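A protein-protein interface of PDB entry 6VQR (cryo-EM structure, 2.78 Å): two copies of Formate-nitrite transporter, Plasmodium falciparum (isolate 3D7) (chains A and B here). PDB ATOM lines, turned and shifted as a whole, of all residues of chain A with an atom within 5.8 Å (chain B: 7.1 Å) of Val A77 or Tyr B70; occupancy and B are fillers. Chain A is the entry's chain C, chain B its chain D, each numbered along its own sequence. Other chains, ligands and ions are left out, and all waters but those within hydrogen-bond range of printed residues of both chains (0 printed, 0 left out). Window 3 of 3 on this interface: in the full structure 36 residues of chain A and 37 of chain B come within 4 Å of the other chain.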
ATOM      1  N   PHE A  68     -18.750 -13.741  -5.660  1.00  0.00           N
ATOM      2  CA  PHE A  68     -17.326 -14.016  -5.550  1.00  0.00           C
ATOM      3  C   PHE A  68     -16.535 -12.832  -5.031  1.00  0.00           C
ATOM      4  O   PHE A  68     -15.316 -12.932  -4.892  1.00  0.00           O
ATOM      5  CB  PHE A  68     -16.769 -14.450  -6.902  1.00  0.00           C
ATOM      6  CG  PHE A  68     -16.969 -15.903  -7.193  1.00  0.00           C
ATOM      7  CD1 PHE A  68     -18.139 -16.351  -7.771  1.00  0.00           C
ATOM      8  CD2 PHE A  68     -15.992 -16.824  -6.879  1.00  0.00           C
ATOM      9  CE1 PHE A  68     -18.326 -17.686  -8.031  1.00  0.00           C
ATOM     10  CE2 PHE A  68     -16.176 -18.157  -7.141  1.00  0.00           C
ATOM     11  CZ  PHE A  68     -17.342 -18.587  -7.720  1.00  0.00           C
ATOM     12  N   LEU A  73     -12.355 -13.475   0.309  1.00  0.00           N
ATOM     13  CA  LEU A  73     -12.002 -13.932  -1.029  1.00  0.00           C
ATOM     14  C   LEU A  73     -11.340 -12.806  -1.806  1.00  0.00           C
ATOM     15  O   LEU A  73     -10.370 -13.022  -2.518  1.00  0.00           O
ATOM     16  CB  LEU A  73     -13.227 -14.422  -1.779  1.00  0.00           C
ATOM     17  CG  LEU A  73     -12.835 -15.027  -3.117  1.00  0.00           C
ATOM     18  CD1 LEU A  73     -11.698 -16.008  -2.901  1.00  0.00           C
ATOM     19  CD2 LEU A  73     -14.016 -15.706  -3.784  1.00  0.00           C
ATOM     20  N   ARG A  74     -11.865 -11.593  -1.641  1.00  0.00           N
ATOM     21  CA  ARG A  74     -11.347 -10.384  -2.268  1.00  0.00           C
ATOM     22  C   ARG A  74      -9.934 -10.087  -1.824  1.00  0.00           C
ATOM     23  O   ARG A  74      -9.155  -9.561  -2.606  1.00  0.00           O
ATOM     24  CB  ARG A  74     -12.228  -9.174  -1.987  1.00  0.00           C
ATOM     25  CG  ARG A  74     -12.969  -8.648  -3.202  1.00  0.00           C
ATOM     26  CD  ARG A  74     -13.500  -7.249  -2.939  1.00  0.00           C
ATOM     27  NE  ARG A  74     -14.226  -7.198  -1.679  1.00  0.00           N
ATOM     28  CZ  ARG A  74     -14.466  -6.086  -1.001  1.00  0.00           C
ATOM     29  NH1 ARG A  74     -14.027  -4.926  -1.460  1.00  0.00           N
ATOM     30  NH2 ARG A  74     -15.134  -6.132   0.138  1.00  0.00           N
ATOM     31  N   GLU A  75      -9.587 -10.379  -0.575  1.00  0.00           N
ATOM     32  CA  GLU A  75      -8.193 -10.101  -0.172  1.00  0.00           C
ATOM     33  C   GLU A  75      -7.027 -10.826  -0.929  1.00  0.00           C
ATOM     34  O   GLU A  75      -5.897 -10.365  -0.872  1.00  0.00           O
ATOM     35  CB  GLU A  75      -8.025 -10.295   1.333  1.00  0.00           C
ATOM     36  CG  GLU A  75      -8.640  -9.186   2.161  1.00  0.00           C
ATOM     37  CD  GLU A  75      -8.593  -9.473   3.648  1.00  0.00           C
ATOM     38  OE1 GLU A  75      -8.385 -10.643   4.023  1.00  0.00           O
ATOM     39  OE2 GLU A  75      -8.770  -8.528   4.444  1.00  0.00           O
ATOM     40  N   ILE A  76      -7.297 -11.949  -1.593  1.00  0.00           N
ATOM     41  CA  ILE A  76      -6.346 -12.806  -2.284  1.00  0.00           C
ATOM     42  C   ILE A  76      -6.480 -12.601  -3.785  1.00  0.00           C
ATOM     43  O   ILE A  76      -5.528 -12.190  -4.454  1.00  0.00           O
ATOM     44  CB  ILE A  76      -6.548 -14.280  -1.906  1.00  0.00           C
ATOM     45  CG1 ILE A  76      -6.061 -14.531  -0.485  1.00  0.00           C
ATOM     46  CG2 ILE A  76      -5.808 -15.178  -2.870  1.00  0.00           C
ATOM     47  CD1 ILE A  76      -6.338 -15.927   0.009  1.00  0.00           C
ATOM     48  N   VAL A  77      -7.646 -12.971  -4.306  1.00  0.00           N
ATOM     49  CA  VAL A  77      -7.977 -12.839  -5.719  1.00  0.00           C
ATOM     50  C   VAL A  77      -8.052 -11.392  -6.199  1.00  0.00           C
ATOM     51  O   VAL A  77      -7.723 -11.100  -7.340  1.00  0.00           O
ATOM     52  CB  VAL A  77      -9.239 -13.627  -6.100  1.00  0.00           C
ATOM     53  CG1 VAL A  77      -9.018 -15.107  -5.846  1.00  0.00           C
ATOM     54  CG2 VAL A  77     -10.449 -13.123  -5.335  1.00  0.00           C
ATOM     55  N   GLY A  78      -8.538 -10.498  -5.350  1.00  0.00           N
ATOM     56  CA  GLY A  78      -8.628  -9.098  -5.711  1.00  0.00           C
ATOM     57  C   GLY A  78      -9.393  -8.810  -6.982  1.00  0.00           C
ATOM     58  O   GLY A  78      -8.862  -8.139  -7.866  1.00  0.00           O
ATOM     59  N   ALA A  79     -10.609  -9.331  -7.101  1.00  0.00           N
ATOM     60  CA  ALA A  79     -11.443  -9.086  -8.280  1.00  0.00           C
ATOM     61  C   ALA A  79     -11.195  -9.952  -9.518  1.00  0.00           C
ATOM     62  O   ALA A  79     -11.753  -9.677 -10.569  1.00  0.00           O
ATOM     63  CB  ALA A  79     -11.373  -7.619  -8.666  1.00  0.00           C
ATOM     64  N   SER A  80     -10.379 -10.992  -9.413  1.00  0.00           N
ATOM     65  CA  SER A  80     -10.117 -11.819 -10.574  1.00  0.00           C
ATOM     66  C   SER A  80     -11.304 -12.722 -10.891  1.00  0.00           C
ATOM     67  O   SER A  80     -11.673 -12.887 -12.047  1.00  0.00           O
ATOM     68  CB  SER A  80      -8.863 -12.658 -10.357  1.00  0.00           C
ATOM     69  OG  SER A  80      -9.140 -13.790  -9.560  1.00  0.00           O
ATOM     70  N   MET A  81     -11.900 -13.296  -9.849  1.00  0.00           N
ATOM     71  CA  MET A  81     -13.030 -14.205  -9.973  1.00  0.00           C
ATOM     72  C   MET A  81     -14.327 -13.453 -10.202  1.00  0.00           C
ATOM     73  O   MET A  81     -15.205 -13.943 -10.915  1.00  0.00           O
ATOM     74  CB  MET A  81     -13.136 -15.083  -8.734  1.00  0.00           C
ATOM     75  CG  MET A  81     -11.810 -15.624  -8.259  1.00  0.00           C
ATOM     76  SD  MET A  81     -11.873 -17.394  -7.950  1.00  0.00           S
ATOM     77  CE  MET A  81     -12.182 -18.000  -9.606  1.00  0.00           C
ATOM     78  N   GLY B  65      -5.579 -11.487 -18.354  1.00  0.00           N
ATOM     79  CA  GLY B  65      -4.423 -12.036 -17.666  1.00  0.00           C
ATOM     80  C   GLY B  65      -3.946 -11.150 -16.534  1.00  0.00           C
ATOM     81  O   GLY B  65      -3.658 -11.624 -15.434  1.00  0.00           O
ATOM     82  N   GLY B  66      -3.842  -9.848 -16.791  1.00  0.00           N
ATOM     83  CA  GLY B  66      -3.490  -8.927 -15.731  1.00  0.00           C
ATOM     84  C   GLY B  66      -4.519  -8.874 -14.630  1.00  0.00           C
ATOM     85  O   GLY B  66      -4.192  -8.512 -13.497  1.00  0.00           O
ATOM     86  N   LEU B  67      -5.766  -9.217 -14.943  1.00  0.00           N
ATOM     87  CA  LEU B  67      -6.779  -9.352 -13.907  1.00  0.00           C
ATOM     88  C   LEU B  67      -6.454 -10.517 -12.996  1.00  0.00           C
ATOM     89  O   LEU B  67      -6.513 -10.395 -11.769  1.00  0.00           O
ATOM     90  CB  LEU B  67      -8.145  -9.545 -14.547  1.00  0.00           C
ATOM     91  CG  LEU B  67      -9.353  -9.133 -13.734  1.00  0.00           C
ATOM     92  CD1 LEU B  67      -9.156  -7.748 -13.144  1.00  0.00           C
ATOM     93  CD2 LEU B  67     -10.527  -9.151 -14.667  1.00  0.00           C
ATOM     94  N   PHE B  68      -6.106 -11.654 -13.581  1.00  0.00           N
ATOM     95  CA  PHE B  68      -5.748 -12.812 -12.769  1.00  0.00           C
ATOM     96  C   PHE B  68      -4.306 -12.791 -12.296  1.00  0.00           C
ATOM     97  O   PHE B  68      -3.852 -13.777 -11.715  1.00  0.00           O
ATOM     98  CB  PHE B  68      -6.018 -14.103 -13.532  1.00  0.00           C
ATOM     99  CG  PHE B  68      -7.351 -14.690 -13.237  1.00  0.00           C
ATOM    100  CD1 PHE B  68      -7.520 -15.545 -12.169  1.00  0.00           C
ATOM    101  CD2 PHE B  68      -8.445 -14.367 -14.009  1.00  0.00           C
ATOM    102  CE1 PHE B  68      -8.750 -16.078 -11.889  1.00  0.00           C
ATOM    103  CE2 PHE B  68      -9.674 -14.899 -13.735  1.00  0.00           C
ATOM    104  CZ  PHE B  68      -9.829 -15.756 -12.674  1.00  0.00           C
ATOM    105  N   TYR B  69      -3.576 -11.702 -12.529  1.00  0.00           N
ATOM    106  CA  TYR B  69      -2.181 -11.585 -12.126  1.00  0.00           C
ATOM    107  C   TYR B  69      -2.003 -10.717 -10.887  1.00  0.00           C
ATOM    108  O   TYR B  69      -0.985 -10.034 -10.756  1.00  0.00           O
ATOM    109  CB  TYR B  69      -1.351 -11.027 -13.282  1.00  0.00           C
ATOM    110  CG  TYR B  69       0.084 -11.500 -13.303  1.00  0.00           C
ATOM    111  CD1 TYR B  69       0.389 -12.851 -13.247  1.00  0.00           C
ATOM    112  CD2 TYR B  69       1.131 -10.600 -13.390  1.00  0.00           C
ATOM    113  CE1 TYR B  69       1.687 -13.286 -13.267  1.00  0.00           C
ATOM    114  CE2 TYR B  69       2.430 -11.032 -13.409  1.00  0.00           C
ATOM    115  CZ  TYR B  69       2.700 -12.375 -13.350  1.00  0.00           C
ATOM    116  OH  TYR B  69       3.997 -12.815 -13.369  1.00  0.00           O
ATOM    117  N   TYR B  70      -2.968 -10.742  -9.973  1.00  0.00           N
ATOM    118  CA  TYR B  70      -2.967  -9.854  -8.819  1.00  0.00           C
ATOM    119  C   TYR B  70      -1.698 -10.030  -7.992  1.00  0.00           C
ATOM    120  O   TYR B  70      -0.960 -11.002  -8.134  1.00  0.00           O
ATOM    121  CB  TYR B  70      -4.204 -10.111  -7.958  1.00  0.00           C
ATOM    122  CG  TYR B  70      -4.417  -9.119  -6.838  1.00  0.00           C
ATOM    123  CD1 TYR B  70      -4.542  -7.771  -7.098  1.00  0.00           C
ATOM    124  CD2 TYR B  70      -4.501  -9.535  -5.525  1.00  0.00           C
ATOM    125  CE1 TYR B  70      -4.734  -6.873  -6.086  1.00  0.00           C
ATOM    126  CE2 TYR B  70      -4.692  -8.643  -4.512  1.00  0.00           C
ATOM    127  CZ  TYR B  70      -4.807  -7.314  -4.797  1.00  0.00           C
ATOM    128  OH  TYR B  70      -5.002  -6.414  -3.782  1.00  0.00           O
ATOM    129  N   HIS B  71      -1.448  -9.059  -7.119  1.00  0.00           N
ATOM    130  CA  HIS B  71      -0.238  -9.071  -6.307  1.00  0.00           C
ATOM    131  C   HIS B  71      -0.182 -10.301  -5.416  1.00  0.00           C
ATOM    132  O   HIS B  71       0.826 -11.011  -5.387  1.00  0.00           O
ATOM    133  CB  HIS B  71      -0.173  -7.797  -5.471  1.00  0.00           C
ATOM    134  CG  HIS B  71       0.818  -7.857  -4.358  1.00  0.00           C
ATOM    135  ND1 HIS B  71       0.575  -7.306  -3.119  1.00  0.00           N
ATOM    136  CD2 HIS B  71       2.060  -8.392  -4.295  1.00  0.00           C
ATOM    137  CE1 HIS B  71       1.622  -7.505  -2.339  1.00  0.00           C
ATOM    138  NE2 HIS B  71       2.537  -8.163  -3.028  1.00  0.00           N
ATOM    139  N   LYS B  72      -1.251 -10.561  -4.668  1.00  0.00           N
ATOM    140  CA  LYS B  72      -1.294 -11.684  -3.740  1.00  0.00           C
ATOM    141  C   LYS B  72      -1.672 -12.993  -4.409  1.00  0.00           C
ATOM    142  O   LYS B  72      -1.644 -14.034  -3.749  1.00  0.00           O
ATOM    143  CB  LYS B  72      -2.279 -11.402  -2.610  1.00  0.00           C
ATOM    144  CG  LYS B  72      -2.048 -10.093  -1.894  1.00  0.00           C
ATOM    145  CD  LYS B  72      -0.822 -10.170  -1.026  1.00  0.00           C
ATOM    146  CE  LYS B  72      -0.805  -9.052  -0.012  1.00  0.00           C
ATOM    147  NZ  LYS B  72       0.408  -9.117   0.848  1.00  0.00           N
ATOM    148  N   LEU B  73      -2.047 -12.962  -5.687  1.00  0.00           N
ATOM    149  CA  LEU B  73      -2.298 -14.192  -6.423  1.00  0.00           C
ATOM    150  C   LEU B  73      -1.014 -14.787  -6.971  1.00  0.00           C
ATOM    151  O   LEU B  73      -0.927 -16.003  -7.142  1.00  0.00           O
ATOM    152  CB  LEU B  73      -3.272 -13.936  -7.569  1.00  0.00           C
ATOM    153  CG  LEU B  73      -4.638 -14.609  -7.500  1.00  0.00           C
ATOM    154  CD1 LEU B  73      -5.387 -14.386  -8.793  1.00  0.00           C
ATOM    155  CD2 LEU B  73      -4.495 -16.086  -7.220  1.00  0.00           C
ATOM    156  N   ARG B  74      -0.020 -13.949  -7.262  1.00  0.00           N
ATOM    157  CA  ARG B  74       1.273 -14.455  -7.704  1.00  0.00           C
ATOM    158  C   ARG B  74       1.986 -15.197  -6.587  1.00  0.00           C
ATOM    159  O   ARG B  74       2.625 -16.226  -6.830  1.00  0.00           O
ATOM    160  CB  ARG B  74       2.146 -13.307  -8.198  1.00  0.00           C
ATOM    161  CG  ARG B  74       1.723 -12.731  -9.512  1.00  0.00           C
ATOM    162  CD  ARG B  74       2.709 -11.692  -9.960  1.00  0.00           C
ATOM    163  NE  ARG B  74       2.729 -10.562  -9.049  1.00  0.00           N
ATOM    164  CZ  ARG B  74       3.300  -9.401  -9.329  1.00  0.00           C
ATOM    165  NH1 ARG B  74       3.894  -9.229 -10.499  1.00  0.00           N
ATOM    166  NH2 ARG B  74       3.280  -8.417  -8.443  1.00  0.00           N
ATOM    167  N   GLU B  75       1.892 -14.693  -5.358  1.00  0.00           N
ATOM    168  CA  GLU B  75       2.650 -15.258  -4.254  1.00  0.00           C
ATOM    169  C   GLU B  75       2.347 -16.728  -4.015  1.00  0.00           C
ATOM    170  O   GLU B  75       3.092 -17.384  -3.281  1.00  0.00           O
ATOM    171  CB  GLU B  75       2.375 -14.457  -2.985  1.00  0.00           C
ATOM    172  CG  GLU B  75       3.280 -13.246  -2.779  1.00  0.00           C
ATOM    173  CD  GLU B  75       4.719 -13.596  -2.411  1.00  0.00           C
ATOM    174  OE1 GLU B  75       5.226 -14.664  -2.815  1.00  0.00           O
ATOM    175  OE2 GLU B  75       5.353 -12.785  -1.703  1.00  0.00           O
ATOM    176  N   SER B  82      -2.865 -16.726 -14.758  1.00  0.00           N
ATOM    177  CA  SER B  82      -2.788 -15.673 -15.763  1.00  0.00           C
ATOM    178  C   SER B  82      -2.598 -16.257 -17.155  1.00  0.00           C
ATOM    179  O   SER B  82      -3.270 -15.853 -18.113  1.00  0.00           O
ATOM    180  CB  SER B  82      -1.650 -14.720 -15.424  1.00  0.00           C
ATOM    181  OG  SER B  82      -1.921 -13.420 -15.906  1.00  0.00           O
ATOM    182  N   VAL B 161       2.053  -0.912  -6.217  1.00  0.00           N
ATOM    183  CA  VAL B 161       2.079  -2.341  -6.499  1.00  0.00           C
ATOM    184  C   VAL B 161       0.711  -2.989  -6.404  1.00  0.00           C
ATOM    185  O   VAL B 161       0.548  -4.128  -6.850  1.00  0.00           O
ATOM    186  CB  VAL B 161       3.057  -3.062  -5.552  1.00  0.00           C
ATOM    187  CG1 VAL B 161       2.384  -3.379  -4.233  1.00  0.00           C
ATOM    188  CG2 VAL B 161       3.593  -4.324  -6.198  1.00  0.00           C
ATOM    189  N   GLU B 162      -0.280  -2.296  -5.842  1.00  0.00           N
ATOM    190  CA  GLU B 162      -1.608  -2.887  -5.710  1.00  0.00           C
ATOM    191  C   GLU B 162      -2.344  -2.894  -7.041  1.00  0.00           C
ATOM    192  O   GLU B 162      -2.987  -3.885  -7.396  1.00  0.00           O
ATOM    193  CB  GLU B 162      -2.432  -2.136  -4.663  1.00  0.00           C
ATOM    194  CG  GLU B 162      -1.896  -2.138  -3.230  1.00  0.00           C
ATOM    195  CD  GLU B 162      -0.539  -1.480  -3.079  1.00  0.00           C
ATOM    196  OE1 GLU B 162      -0.291  -0.466  -3.763  1.00  0.00           O
ATOM    197  OE2 GLU B 162       0.273  -1.966  -2.265  1.00  0.00           O
ATOM    198  N   LYS B 163      -2.258  -1.800  -7.790  1.00  0.00           N
ATOM    199  CA  LYS B 163      -2.983  -1.645  -9.040  1.00  0.00           C
ATOM    200  C   LYS B 163      -2.165  -2.043 -10.258  1.00  0.00           C
ATOM    201  O   LYS B 163      -2.734  -2.215 -11.340  1.00  0.00           O
ATOM    202  CB  LYS B 163      -3.456  -0.195  -9.219  1.00  0.00           C
ATOM    203  CG  LYS B 163      -4.092   0.464  -7.993  1.00  0.00           C
ATOM    204  CD  LYS B 163      -3.060   1.003  -7.011  1.00  0.00           C
ATOM    205  CE  LYS B 163      -3.716   1.596  -5.781  1.00  0.00           C
ATOM    206  NZ  LYS B 163      -2.924   1.307  -4.555  1.00  0.00           N
ATOM    207  N   HIS B 165      -1.091  -4.659 -11.314  1.00  0.00           N
ATOM    208  CA  HIS B 165      -1.181  -6.029 -11.800  1.00  0.00           C
ATOM    209  C   HIS B 165      -1.425  -6.109 -13.296  1.00  0.00           C
ATOM    210  O   HIS B 165      -1.449  -7.216 -13.839  1.00  0.00           O
ATOM    211  CB  HIS B 165      -2.287  -6.780 -11.061  1.00  0.00           C
ATOM    212  CG  HIS B 165      -3.579  -6.033 -10.991  1.00  0.00           C
ATOM    213  ND1 HIS B 165      -3.791  -4.996 -10.112  1.00  0.00           N
ATOM    214  CD2 HIS B 165      -4.726  -6.171 -11.695  1.00  0.00           C
ATOM    215  CE1 HIS B 165      -5.013  -4.524 -10.278  1.00  0.00           C
ATOM    216  NE2 HIS B 165      -5.601  -5.219 -11.233  1.00  0.00           N
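Among the printed residues, merely in contact across the chains: Glu A75 with Lys B72 (3.99 Å), Ile A76 with Tyr B70 (3.0 Å), Ile A76 with Lys B72 (3.8 Å), Ile A76 with Leu B73 (3.8 Å), Val A77 with Tyr B70 (3.7 Å), Ser A80 with Leu B67 (3.6 Å), Ser A80 with Phe B68 (3.3 Å) and Ser A80 with Leu B73 (3.9 Å).
Of the printed residues of chain B, Glu A75 touches Lys B72 (3.99 Å). Printed residues of chain B within 4 Å of Ile A76: Tyr B70 (3.0 Å), Lys B72 (3.8 Å) and Leu B73 (3.8 Å). Of chain B, only Tyr B70 (3.7 Å) comes within 4 Å of Val A77. Of the printed residues of chain A, Leu B67 touches Ser A80. Tyr B69 touches none of the printed residues of chain A. Of the printed residues of chain A, Lys B72 touches Glu A75 and Ile A76. Glu B75 touches none of the printed residues of chain A. The nearest residue of chain A that does not touch Tyr B70 is Gly A78 (4.1 Å). The nearest printed residue of chain B that does not touch Ile A76 is His B71 (5.8 Å).
Of the 16 printed residues of chain B, 5 touch a printed residue of chain A. Hydrophobic or aromatic side chains of chain B within 4 Å of the printed part of chain A: Phe B68, Tyr B70 and Leu B73. Of the 10 printed residues of chain A, 4 touch a printed residue of chain B. Printed residues of chain A that touch a printed residue of chain B: Glu A75, Ile A76, Val A77 and Ser A80. Among the printed residues, 8 pairs touch across the chains. Among the printed residues, no Asp or Glu carboxylate lies within 4 Å of a Lys or Arg side-chain nitrogen of the other chain.
Positions printed for both chains: 68, 73, 74 and 75.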
